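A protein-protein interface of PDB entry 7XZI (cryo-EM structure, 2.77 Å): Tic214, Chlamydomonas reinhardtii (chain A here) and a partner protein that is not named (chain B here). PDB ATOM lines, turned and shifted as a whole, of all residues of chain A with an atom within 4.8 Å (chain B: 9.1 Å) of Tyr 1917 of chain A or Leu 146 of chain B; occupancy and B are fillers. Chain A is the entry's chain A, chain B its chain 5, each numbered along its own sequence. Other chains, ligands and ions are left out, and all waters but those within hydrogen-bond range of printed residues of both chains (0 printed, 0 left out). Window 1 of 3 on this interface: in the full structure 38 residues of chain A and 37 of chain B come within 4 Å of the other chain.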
ATOM      1  N   HIS A  21       2.353  11.815 -22.449  1.00  0.00           N
ATOM      2  CA  HIS A  21       3.728  11.950 -22.921  1.00  0.00           C
ATOM      3  C   HIS A  21       4.072  13.405 -23.212  1.00  0.00           C
ATOM      4  O   HIS A  21       5.207  13.839 -22.985  1.00  0.00           O
ATOM      5  CB  HIS A  21       3.947  11.090 -24.166  1.00  0.00           C
ATOM      6  CG  HIS A  21       4.025   9.624 -23.880  1.00  0.00           C
ATOM      7  ND1 HIS A  21       4.122   8.676 -24.875  1.00  0.00           N
ATOM      8  CD2 HIS A  21       4.025   8.942 -22.710  1.00  0.00           C
ATOM      9  CE1 HIS A  21       4.175   7.474 -24.332  1.00  0.00           C
ATOM     10  NE2 HIS A  21       4.119   7.608 -23.019  1.00  0.00           N
ATOM     11  N   ASN A1624      17.657   4.090 -29.053  1.00  0.00           N
ATOM     12  CA  ASN A1624      18.289   4.171 -27.739  1.00  0.00           C
ATOM     13  C   ASN A1624      17.936   2.932 -26.927  1.00  0.00           C
ATOM     14  O   ASN A1624      17.366   1.980 -27.467  1.00  0.00           O
ATOM     15  CB  ASN A1624      17.866   5.443 -27.002  1.00  0.00           C
ATOM     16  CG  ASN A1624      16.365   5.564 -26.855  1.00  0.00           C
ATOM     17  OD1 ASN A1624      15.767   4.974 -25.955  1.00  0.00           O
ATOM     18  ND2 ASN A1624      15.746   6.338 -27.738  1.00  0.00           N
ATOM     19  N   GLU A1625      18.273   2.929 -25.636  1.00  0.00           N
ATOM     20  CA  GLU A1625      18.064   1.741 -24.812  1.00  0.00           C
ATOM     21  C   GLU A1625      16.582   1.393 -24.701  1.00  0.00           C
ATOM     22  O   GLU A1625      16.177   0.253 -24.956  1.00  0.00           O
ATOM     23  CB  GLU A1625      18.677   1.952 -23.426  1.00  0.00           C
ATOM     24  CG  GLU A1625      20.195   1.856 -23.390  1.00  0.00           C
ATOM     25  CD  GLU A1625      20.695   0.423 -23.426  1.00  0.00           C
ATOM     26  OE1 GLU A1625      19.860  -0.504 -23.361  1.00  0.00           O
ATOM     27  OE2 GLU A1625      21.925   0.222 -23.514  1.00  0.00           O
ATOM     28  N   GLY A1626      15.755   2.368 -24.318  1.00  0.00           N
ATOM     29  CA  GLY A1626      14.331   2.102 -24.183  1.00  0.00           C
ATOM     30  C   GLY A1626      13.665   1.787 -25.509  1.00  0.00           C
ATOM     31  O   GLY A1626      12.839   0.873 -25.601  1.00  0.00           O
ATOM     32  N   SER A1627      14.012   2.542 -26.554  1.00  0.00           N
ATOM     33  CA  SER A1627      13.450   2.283 -27.875  1.00  0.00           C
ATOM     34  C   SER A1627      13.839   0.898 -28.377  1.00  0.00           C
ATOM     35  O   SER A1627      13.012   0.187 -28.960  1.00  0.00           O
ATOM     36  CB  SER A1627      13.909   3.362 -28.855  1.00  0.00           C
ATOM     37  OG  SER A1627      13.402   3.121 -30.154  1.00  0.00           O
ATOM     38  N   TYR A1630      11.762  -1.663 -26.573  1.00  0.00           N
ATOM     39  CA  TYR A1630      10.367  -1.742 -26.993  1.00  0.00           C
ATOM     40  C   TYR A1630      10.209  -2.537 -28.285  1.00  0.00           C
ATOM     41  O   TYR A1630       9.268  -3.326 -28.418  1.00  0.00           O
ATOM     42  CB  TYR A1630       9.788  -0.337 -27.156  1.00  0.00           C
ATOM     43  CG  TYR A1630       8.276  -0.295 -27.160  1.00  0.00           C
ATOM     44  CD1 TYR A1630       7.556  -0.572 -26.007  1.00  0.00           C
ATOM     45  CD2 TYR A1630       7.571   0.028 -28.310  1.00  0.00           C
ATOM     46  CE1 TYR A1630       6.176  -0.535 -26.000  1.00  0.00           C
ATOM     47  CE2 TYR A1630       6.189   0.070 -28.313  1.00  0.00           C
ATOM     48  CZ  TYR A1630       5.498  -0.212 -27.154  1.00  0.00           C
ATOM     49  OH  TYR A1630       4.122  -0.174 -27.145  1.00  0.00           O
ATOM     50  N   THR A1912      -0.508   2.877 -27.676  1.00  0.00           N
ATOM     51  CA  THR A1912       0.210   4.054 -28.141  1.00  0.00           C
ATOM     52  C   THR A1912       0.196   4.081 -29.661  1.00  0.00           C
ATOM     53  O   THR A1912       0.023   3.053 -30.320  1.00  0.00           O
ATOM     54  CB  THR A1912       1.658   4.078 -27.634  1.00  0.00           C
ATOM     55  OG1 THR A1912       2.342   5.205 -28.194  1.00  0.00           O
ATOM     56  CG2 THR A1912       2.380   2.804 -28.035  1.00  0.00           C
ATOM     57  N   GLY A1915       4.463   5.732 -33.567  1.00  0.00           N
ATOM     58  CA  GLY A1915       5.706   6.477 -33.463  1.00  0.00           C
ATOM     59  C   GLY A1915       6.444   6.311 -32.151  1.00  0.00           C
ATOM     60  O   GLY A1915       7.668   6.154 -32.148  1.00  0.00           O
ATOM     61  N   ASP A1916       5.731   6.345 -31.030  1.00  0.00           N
ATOM     62  CA  ASP A1916       6.367   6.420 -29.722  1.00  0.00           C
ATOM     63  C   ASP A1916       6.390   5.063 -29.021  1.00  0.00           C
ATOM     64  O   ASP A1916       5.888   4.056 -29.525  1.00  0.00           O
ATOM     65  CB  ASP A1916       5.652   7.448 -28.847  1.00  0.00           C
ATOM     66  CG  ASP A1916       5.604   8.822 -29.485  1.00  0.00           C
ATOM     67  OD1 ASP A1916       6.199   9.001 -30.569  1.00  0.00           O
ATOM     68  OD2 ASP A1916       4.967   9.724 -28.903  1.00  0.00           O
ATOM     69  N   TYR A1917       6.992   5.054 -27.831  1.00  0.00           N
ATOM     70  CA  TYR A1917       7.009   3.909 -26.930  1.00  0.00           C
ATOM     71  C   TYR A1917       6.539   4.367 -25.554  1.00  0.00           C
ATOM     72  O   TYR A1917       6.242   5.545 -25.335  1.00  0.00           O
ATOM     73  CB  TYR A1917       8.404   3.273 -26.855  1.00  0.00           C
ATOM     74  CG  TYR A1917       9.455   4.146 -26.202  1.00  0.00           C
ATOM     75  CD1 TYR A1917      10.112   5.133 -26.924  1.00  0.00           C
ATOM     76  CD2 TYR A1917       9.798   3.975 -24.867  1.00  0.00           C
ATOM     77  CE1 TYR A1917      11.074   5.930 -26.333  1.00  0.00           C
ATOM     78  CE2 TYR A1917      10.758   4.769 -24.268  1.00  0.00           C
ATOM     79  CZ  TYR A1917      11.393   5.743 -25.005  1.00  0.00           C
ATOM     80  OH  TYR A1917      12.350   6.534 -24.411  1.00  0.00           O
ATOM     81  N   LEU A1918       6.476   3.428 -24.611  1.00  0.00           N
ATOM     82  CA  LEU A1918       6.001   3.718 -23.257  1.00  0.00           C
ATOM     83  C   LEU A1918       7.117   4.411 -22.485  1.00  0.00           C
ATOM     84  O   LEU A1918       8.030   3.777 -21.956  1.00  0.00           O
ATOM     85  CB  LEU A1918       5.545   2.443 -22.557  1.00  0.00           C
ATOM     86  CG  LEU A1918       4.292   1.771 -23.123  1.00  0.00           C
ATOM     87  CD1 LEU A1918       3.921   0.541 -22.309  1.00  0.00           C
ATOM     88  CD2 LEU A1918       3.133   2.752 -23.170  1.00  0.00           C
ATOM     89  N   ARG A1919       7.041   5.743 -22.426  1.00  0.00           N
ATOM     90  CA  ARG A1919       8.067   6.519 -21.738  1.00  0.00           C
ATOM     91  C   ARG A1919       7.913   6.456 -20.224  1.00  0.00           C
ATOM     92  O   ARG A1919       8.917   6.431 -19.503  1.00  0.00           O
ATOM     93  CB  ARG A1919       8.027   7.973 -22.202  1.00  0.00           C
ATOM     94  CG  ARG A1919       8.083   8.155 -23.705  1.00  0.00           C
ATOM     95  CD  ARG A1919       7.929   9.618 -24.077  1.00  0.00           C
ATOM     96  NE  ARG A1919       7.871   9.812 -25.517  1.00  0.00           N
ATOM     97  CZ  ARG A1919       7.691  10.988 -26.109  1.00  0.00           C
ATOM     98  NH1 ARG A1919       7.548  12.100 -25.405  1.00  0.00           N
ATOM     99  NH2 ARG A1919       7.653  11.048 -27.436  1.00  0.00           N
ATOM    100  N   SER B 140      11.974   4.550 -10.628  1.00  0.00           N
ATOM    101  CA  SER B 140      12.037   5.699 -11.517  1.00  0.00           C
ATOM    102  C   SER B 140      11.481   5.315 -12.881  1.00  0.00           C
ATOM    103  O   SER B 140      11.426   4.137 -13.244  1.00  0.00           O
ATOM    104  CB  SER B 140      13.471   6.229 -11.656  1.00  0.00           C
ATOM    105  OG  SER B 140      14.336   5.232 -12.170  1.00  0.00           O
ATOM    106  N   LYS B 141      11.060   6.328 -13.631  1.00  0.00           N
ATOM    107  CA  LYS B 141      10.519   6.112 -14.963  1.00  0.00           C
ATOM    108  C   LYS B 141      11.645   5.898 -15.973  1.00  0.00           C
ATOM    109  O   LYS B 141      12.811   6.210 -15.720  1.00  0.00           O
ATOM    110  CB  LYS B 141       9.635   7.289 -15.377  1.00  0.00           C
ATOM    111  CG  LYS B 141       8.299   7.331 -14.645  1.00  0.00           C
ATOM    112  CD  LYS B 141       7.511   8.590 -14.966  1.00  0.00           C
ATOM    113  CE  LYS B 141       8.029   9.789 -14.187  1.00  0.00           C
ATOM    114  NZ  LYS B 141       7.843   9.621 -12.721  1.00  0.00           N
ATOM    115  N   VAL B 142      11.275   5.346 -17.131  1.00  0.00           N
ATOM    116  CA  VAL B 142      12.267   4.944 -18.126  1.00  0.00           C
ATOM    117  C   VAL B 142      13.037   6.152 -18.650  1.00  0.00           C
ATOM    118  O   VAL B 142      14.264   6.101 -18.809  1.00  0.00           O
ATOM    119  CB  VAL B 142      11.592   4.161 -19.268  1.00  0.00           C
ATOM    120  CG1 VAL B 142      12.595   3.842 -20.363  1.00  0.00           C
ATOM    121  CG2 VAL B 142      10.969   2.883 -18.733  1.00  0.00           C
ATOM    122  N   TYR B 143      12.338   7.253 -18.937  1.00  0.00           N
ATOM    123  CA  TYR B 143      13.020   8.426 -19.477  1.00  0.00           C
ATOM    124  C   TYR B 143      13.969   9.030 -18.449  1.00  0.00           C
ATOM    125  O   TYR B 143      15.027   9.559 -18.806  1.00  0.00           O
ATOM    126  CB  TYR B 143      12.005   9.462 -19.962  1.00  0.00           C
ATOM    127  CG  TYR B 143      11.300  10.224 -18.865  1.00  0.00           C
ATOM    128  CD1 TYR B 143      10.187   9.694 -18.233  1.00  0.00           C
ATOM    129  CD2 TYR B 143      11.742  11.481 -18.470  1.00  0.00           C
ATOM    130  CE1 TYR B 143       9.538  10.389 -17.233  1.00  0.00           C
ATOM    131  CE2 TYR B 143      11.099  12.182 -17.471  1.00  0.00           C
ATOM    132  CZ  TYR B 143       9.996  11.630 -16.856  1.00  0.00           C
ATOM    133  OH  TYR B 143       9.349  12.323 -15.858  1.00  0.00           O
ATOM    134  N   GLU B 144      13.616   8.952 -17.164  1.00  0.00           N
ATOM    135  CA  GLU B 144      14.540   9.385 -16.119  1.00  0.00           C
ATOM    136  C   GLU B 144      15.789   8.514 -16.096  1.00  0.00           C
ATOM    137  O   GLU B 144      16.905   9.017 -15.907  1.00  0.00           O
ATOM    138  CB  GLU B 144      13.840   9.365 -14.760  1.00  0.00           C
ATOM    139  CG  GLU B 144      12.647  10.304 -14.667  1.00  0.00           C
ATOM    140  CD  GLU B 144      11.952  10.237 -13.320  1.00  0.00           C
ATOM    141  OE1 GLU B 144      12.211   9.282 -12.561  1.00  0.00           O
ATOM    142  OE2 GLU B 144      11.147  11.145 -13.021  1.00  0.00           O
ATOM    143  N   VAL B 145      15.623   7.204 -16.288  1.00  0.00           N
ATOM    144  CA  VAL B 145      16.775   6.309 -16.355  1.00  0.00           C
ATOM    145  C   VAL B 145      17.657   6.667 -17.544  1.00  0.00           C
ATOM    146  O   VAL B 145      18.888   6.702 -17.433  1.00  0.00           O
ATOM    147  CB  VAL B 145      16.309   4.843 -16.413  1.00  0.00           C
ATOM    148  CG1 VAL B 145      17.494   3.919 -16.614  1.00  0.00           C
ATOM    149  CG2 VAL B 145      15.561   4.481 -15.142  1.00  0.00           C
ATOM    150  N   LEU B 146      17.045   6.942 -18.697  1.00  0.00           N
ATOM    151  CA  LEU B 146      17.820   7.349 -19.865  1.00  0.00           C
ATOM    152  C   LEU B 146      18.541   8.670 -19.629  1.00  0.00           C
ATOM    153  O   LEU B 146      19.665   8.855 -20.110  1.00  0.00           O
ATOM    154  CB  LEU B 146      16.914   7.454 -21.093  1.00  0.00           C
ATOM    155  CG  LEU B 146      16.344   6.153 -21.660  1.00  0.00           C
ATOM    156  CD1 LEU B 146      15.479   6.438 -22.879  1.00  0.00           C
ATOM    157  CD2 LEU B 146      17.463   5.185 -22.009  1.00  0.00           C
ATOM    158  N   GLN B 147      17.912   9.598 -18.905  1.00  0.00           N
ATOM    159  CA  GLN B 147      18.558  10.871 -18.606  1.00  0.00           C
ATOM    160  C   GLN B 147      19.727  10.709 -17.642  1.00  0.00           C
ATOM    161  O   GLN B 147      20.732  11.417 -17.771  1.00  0.00           O
ATOM    162  CB  GLN B 147      17.543  11.855 -18.021  1.00  0.00           C
ATOM    163  CG  GLN B 147      16.513  12.374 -19.006  1.00  0.00           C
ATOM    164  CD  GLN B 147      15.553  13.359 -18.368  1.00  0.00           C
ATOM    165  OE1 GLN B 147      15.609  13.604 -17.164  1.00  0.00           O
ATOM    166  NE2 GLN B 147      14.668  13.931 -19.175  1.00  0.00           N
ATOM    167  N   ASN B 148      19.619   9.799 -16.675  1.00  0.00           N
ATOM    168  CA  ASN B 148      20.594   9.772 -15.590  1.00  0.00           C
ATOM    169  C   ASN B 148      21.632   8.665 -15.734  1.00  0.00           C
ATOM    170  O   ASN B 148      22.836   8.938 -15.759  1.00  0.00           O
ATOM    171  CB  ASN B 148      19.875   9.629 -14.246  1.00  0.00           C
ATOM    172  CG  ASN B 148      18.912  10.768 -13.974  1.00  0.00           C
ATOM    173  OD1 ASN B 148      19.092  11.881 -14.468  1.00  0.00           O
ATOM    174  ND2 ASN B 148      17.883  10.496 -13.181  1.00  0.00           N
ATOM    175  N   TYR B 149      21.182   7.412 -15.834  1.00  0.00           N
ATOM    176  CA  TYR B 149      22.111   6.290 -15.744  1.00  0.00           C
ATOM    177  C   TYR B 149      22.649   5.879 -17.111  1.00  0.00           C
ATOM    178  O   TYR B 149      23.809   5.463 -17.224  1.00  0.00           O
ATOM    179  CB  TYR B 149      21.429   5.104 -15.062  1.00  0.00           C
ATOM    180  CG  TYR B 149      21.288   5.258 -13.566  1.00  0.00           C
ATOM    181  CD1 TYR B 149      22.315   4.879 -12.713  1.00  0.00           C
ATOM    182  CD2 TYR B 149      20.130   5.779 -13.005  1.00  0.00           C
ATOM    183  CE1 TYR B 149      22.194   5.014 -11.345  1.00  0.00           C
ATOM    184  CE2 TYR B 149      19.999   5.919 -11.635  1.00  0.00           C
ATOM    185  CZ  TYR B 149      21.035   5.534 -10.811  1.00  0.00           C
ATOM    186  OH  TYR B 149      20.913   5.670  -9.447  1.00  0.00           O
ATOM    187  N   THR B 150      21.833   5.982 -18.153  1.00  0.00           N
ATOM    188  CA  THR B 150      22.216   5.442 -19.451  1.00  0.00           C
ATOM    189  C   THR B 150      23.389   6.225 -20.034  1.00  0.00           C
ATOM    190  O   THR B 150      23.321   7.459 -20.123  1.00  0.00           O
ATOM    191  CB  THR B 150      21.033   5.478 -20.418  1.00  0.00           C
ATOM    192  OG1 THR B 150      19.972   4.662 -19.908  1.00  0.00           O
ATOM    193  CG2 THR B 150      21.447   4.960 -21.787  1.00  0.00           C
ATOM    194  N   PRO B 151      24.470   5.561 -20.433  1.00  0.00           N
ATOM    195  CA  PRO B 151      25.578   6.270 -21.080  1.00  0.00           C
ATOM    196  C   PRO B 151      25.191   6.747 -22.471  1.00  0.00           C
ATOM    197  O   PRO B 151      24.272   6.228 -23.108  1.00  0.00           O
ATOM    198  CB  PRO B 151      26.689   5.217 -21.140  1.00  0.00           C
ATOM    199  CG  PRO B 151      25.962   3.915 -21.148  1.00  0.00           C
ATOM    200  CD  PRO B 151      24.747   4.121 -20.285  1.00  0.00           C
ATOM    201  N   ALA B 152      25.919   7.761 -22.943  1.00  0.00           N
ATOM    202  CA  ALA B 152      25.625   8.356 -24.240  1.00  0.00           C
ATOM    203  C   ALA B 152      26.134   7.523 -25.408  1.00  0.00           C
ATOM    204  O   ALA B 152      25.773   7.810 -26.555  1.00  0.00           O
ATOM    205  CB  ALA B 152      26.222   9.763 -24.322  1.00  0.00           C
ATOM    206  N   ALA B 154      25.424   4.407 -26.042  1.00  0.00           N
ATOM    207  CA  ALA B 154      24.414   3.441 -26.474  1.00  0.00           C
ATOM    208  C   ALA B 154      23.266   4.120 -27.213  1.00  0.00           C
ATOM    209  O   ALA B 154      22.096   3.965 -26.864  1.00  0.00           O
ATOM    210  CB  ALA B 154      23.904   2.654 -25.273  1.00  0.00           C
ATOM    211  N   ALA B 155      23.601   4.880 -28.253  1.00  0.00           N
ATOM    212  CA  ALA B 155      22.594   5.598 -29.031  1.00  0.00           C
ATOM    213  C   ALA B 155      23.196   5.985 -30.371  1.00  0.00           C
ATOM    214  O   ALA B 155      24.228   6.663 -30.409  1.00  0.00           O
ATOM    215  CB  ALA B 155      22.105   6.836 -28.282  1.00  0.00           C
ATOM    216  N   ALA B 179      18.234  10.535 -31.977  1.00  0.00           N
ATOM    217  CA  ALA B 179      18.478   9.707 -30.805  1.00  0.00           C
ATOM    218  C   ALA B 179      18.510  10.596 -29.569  1.00  0.00           C
ATOM    219  O   ALA B 179      18.727  11.807 -29.660  1.00  0.00           O
ATOM    220  CB  ALA B 179      19.786   8.916 -30.931  1.00  0.00           C
ATOM    221  N   LEU B 180      18.276   9.985 -28.411  1.00  0.00           N
ATOM    222  CA  LEU B 180      18.335  10.665 -27.115  1.00  0.00           C
ATOM    223  C   LEU B 180      17.666  12.039 -27.184  1.00  0.00           C
ATOM    224  O   LEU B 180      18.294  13.080 -27.000  1.00  0.00           O
ATOM    225  CB  LEU B 180      19.777  10.784 -26.626  1.00  0.00           C
ATOM    226  CG  LEU B 180      20.499   9.496 -26.224  1.00  0.00           C
ATOM    227  CD1 LEU B 180      21.934   9.789 -25.805  1.00  0.00           C
ATOM    228  CD2 LEU B 180      19.749   8.781 -25.110  1.00  0.00           C
ATOM    229  N   ARG B 181      16.368  12.017 -27.482  1.00  0.00           N
ATOM    230  CA  ARG B 181      15.617  13.239 -27.731  1.00  0.00           C
ATOM    231  C   ARG B 181      15.623  14.145 -26.499  1.00  0.00           C
ATOM    232  O   ARG B 181      16.054  13.760 -25.408  1.00  0.00           O
ATOM    233  CB  ARG B 181      14.183  12.914 -28.145  1.00  0.00           C
ATOM    234  CG  ARG B 181      13.986  12.667 -29.637  1.00  0.00           C
ATOM    235  CD  ARG B 181      14.671  11.392 -30.095  1.00  0.00           C
ATOM    236  NE  ARG B 181      14.211  10.228 -29.350  1.00  0.00           N
ATOM    237  CZ  ARG B 181      13.206   9.445 -29.727  1.00  0.00           C
ATOM    238  NH1 ARG B 181      12.523   9.683 -30.835  1.00  0.00           N
ATOM    239  NH2 ARG B 181      12.883   8.398 -28.976  1.00  0.00           N
ATOM    240  N   PHE B 183      13.590  15.101 -24.399  1.00  0.00           N
ATOM    241  CA  PHE B 183      13.019  14.529 -23.185  1.00  0.00           C
ATOM    242  C   PHE B 183      13.840  13.367 -22.635  1.00  0.00           C
ATOM    243  O   PHE B 183      13.565  12.917 -21.518  1.00  0.00           O
ATOM    244  CB  PHE B 183      11.575  14.082 -23.441  1.00  0.00           C
ATOM    245  CG  PHE B 183      11.413  13.168 -24.626  1.00  0.00           C
ATOM    246  CD1 PHE B 183      11.545  11.797 -24.486  1.00  0.00           C
ATOM    247  CD2 PHE B 183      11.107  13.681 -25.877  1.00  0.00           C
ATOM    248  CE1 PHE B 183      11.390  10.955 -25.570  1.00  0.00           C
ATOM    249  CE2 PHE B 183      10.948  12.843 -26.965  1.00  0.00           C
ATOM    250  CZ  PHE B 183      11.092  11.479 -26.811  1.00  0.00           C
ATOM    251  N   GLU B 184      14.833  12.873 -23.378  1.00  0.00           N
ATOM    252  CA  GLU B 184      15.702  11.798 -22.911  1.00  0.00           C
ATOM    253  C   GLU B 184      17.091  12.298 -22.528  1.00  0.00           C
ATOM    254  O   GLU B 184      17.999  11.490 -22.310  1.00  0.00           O
ATOM    255  CB  GLU B 184      15.813  10.700 -23.970  1.00  0.00           C
ATOM    256  CG  GLU B 184      14.520   9.948 -24.220  1.00  0.00           C
ATOM    257  CD  GLU B 184      14.649   8.916 -25.322  1.00  0.00           C
ATOM    258  OE1 GLU B 184      15.764   8.749 -25.857  1.00  0.00           O
ATOM    259  OE2 GLU B 184      13.632   8.271 -25.653  1.00  0.00           O
ATOM    260  N   ARG B 185      17.273  13.612 -22.441  1.00  0.00           N
ATOM    261  CA  ARG B 185      18.541  14.210 -22.045  1.00  0.00           C
ATOM    262  C   ARG B 185      18.324  15.098 -20.829  1.00  0.00           C
ATOM    263  O   ARG B 185      17.307  15.792 -20.728  1.00  0.00           O
ATOM    264  CB  ARG B 185      19.160  15.014 -23.194  1.00  0.00           C
ATOM    265  CG  ARG B 185      19.853  14.148 -24.232  1.00  0.00           C
ATOM    266  CD  ARG B 185      20.465  14.969 -25.357  1.00  0.00           C
ATOM    267  NE  ARG B 185      19.469  15.435 -26.311  1.00  0.00           N
ATOM    268  CZ  ARG B 185      19.023  16.685 -26.381  1.00  0.00           C
ATOM    269  NH1 ARG B 185      19.474  17.626 -25.568  1.00  0.00           N
ATOM    270  NH2 ARG B 185      18.110  16.997 -27.294  1.00  0.00           N
ATOM    271  N   ARG B 186      19.289  15.069 -19.906  1.00  0.00           N
ATOM    272  CA  ARG B 186      19.137  15.769 -18.635  1.00  0.00           C
ATOM    273  C   ARG B 186      19.015  17.278 -18.808  1.00  0.00           C
ATOM    274  O   ARG B 186      18.320  17.926 -18.019  1.00  0.00           O
ATOM    275  CB  ARG B 186      20.317  15.443 -17.718  1.00  0.00           C
ATOM    276  CG  ARG B 186      20.106  15.838 -16.266  1.00  0.00           C
ATOM    277  CD  ARG B 186      21.347  15.581 -15.419  1.00  0.00           C
ATOM    278  NE  ARG B 186      21.753  14.182 -15.428  1.00  0.00           N
ATOM    279  CZ  ARG B 186      22.786  13.703 -16.114  1.00  0.00           C
ATOM    280  NH1 ARG B 186      23.545  14.489 -16.859  1.00  0.00           N
ATOM    281  NH2 ARG B 186      23.063  12.405 -16.047  1.00  0.00           N
ATOM    282  N   ASP B 187      19.667  17.850 -19.820  1.00  0.00           N
ATOM    283  CA  ASP B 187      19.586  19.282 -20.082  1.00  0.00           C
ATOM    284  C   ASP B 187      18.867  19.592 -21.387  1.00  0.00           C
ATOM    285  O   ASP B 187      18.971  20.717 -21.889  1.00  0.00           O
ATOM    286  CB  ASP B 187      20.986  19.902 -20.093  1.00  0.00           C
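The side-chain amide nitrogen (ND2) of Asn 1624 of chain A sits at hydrogen-bond distance from the side-chain carboxylate (OE1) of Glu 184 of chain B (3.1 Å). OH of Tyr 1917 of chain A sits at hydrogen-bond distance from OE2 of Glu 184 of chain B, 2.5 Å away.
The backbone carbonyl oxygen (O) of Val 145 of chain B lies within hydrogen-bond range of the backbone NH (N) of Thr 150 of chain B, 3.1 Å away. NE2 of Gln 147 of chain B sits at hydrogen-bond distance from O of Phe 183 of chain B (2.8 Å). NH2 of Arg 181 of chain B is in salt-bridge range of OE2 of Glu 184 of chain B, 3.4 Å away. The backbone NH of Gly 1626 of chain A is in hydrogen-bond range of the side-chain amide oxygen of Asn 1624 of chain A. The side-chain amide oxygen (OD1) of Asn 1624 of chain A is in hydrogen-bond range of the backbone NH (N) of Ser 1627 of chain A, 3.1 Å away. NH2 of Arg 1919 of chain A lies within salt-bridge range of OD2 of Asp 1916 of chain A, 3.3 Å away.
OD1 of Asn 1624 of chain A touches CD1 of Leu 146 of chain B (3.4 Å). Ala 154 of chain B touches Asn 1624 of chain A (O to CA, 3.9 Å). Arg 181 of chain B touches Asn 1624 of chain A. Leu 146 of chain B touches Glu 1625 of chain A (CD2 to CB, 3.7 Å). CG of Glu 1625 of chain A touches CG2 of Thr 150 of chain B, 3.7 Å away. Glu 1625 of chain A touches Ala 154 of chain B. Leu 146 of chain B touches Tyr 1917 of chain A (CD1 to OH, 3.5 Å). Arg 1919 of chain A touches Val 142 of chain B (O to CB, 3.5 Å). O of Arg 1919 of chain A touches N of Tyr 143 of chain B, at 3.6 Å. CZ of Arg 1919 of chain A touches CZ of Phe 183 of chain B, 3.5 Å away.
Of the printed residues of chain B, Glu 1625 of chain A touches Leu 146, Thr 150 and Ala 154. No residue of chain B comes within 4 Å of Gly 1626 of chain A. Tyr 1917 of chain A touches two residues of chain B. Leu 146 of chain B touches just these residues of chain A: Asn 1624 (3.4 Å), Glu 1625 (3.7 Å) and Tyr 1917 (3.5 Å). Leu 180 of chain B touches none of the printed residues of chain A. Printed residues of chain A within 4 Å of Phe 183 of chain B: Arg 1919. The nearest residue of chain B that does not touch Tyr 1917 of chain A is Arg 181 of chain B (4.04 Å). The nearest residue of chain A that does not touch Leu 146 of chain B is Gly 1626 of chain A (4.02 Å). The nearest printed residue of chain B that does not touch Arg 1919 of chain A is Lys 141 of chain B (4.3 Å).
Printed residues of chain B that touch a printed residue of chain A: Val 142, Tyr 143, Leu 146, Thr 150, Ala 154, Arg 181, Phe 183 and Glu 184. Hydrophobic or aromatic side chains of chain B within 4 Å of the printed part of chain A: Val 142, Tyr 143, Leu 146, Ala 154 and Phe 183. Of the 12 printed residues of chain A, 4 touch a printed residue of chain B. Printed residues of chain A that touch a printed residue of chain B: Asn 1624, Glu 1625, Tyr 1917 and Arg 1919.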
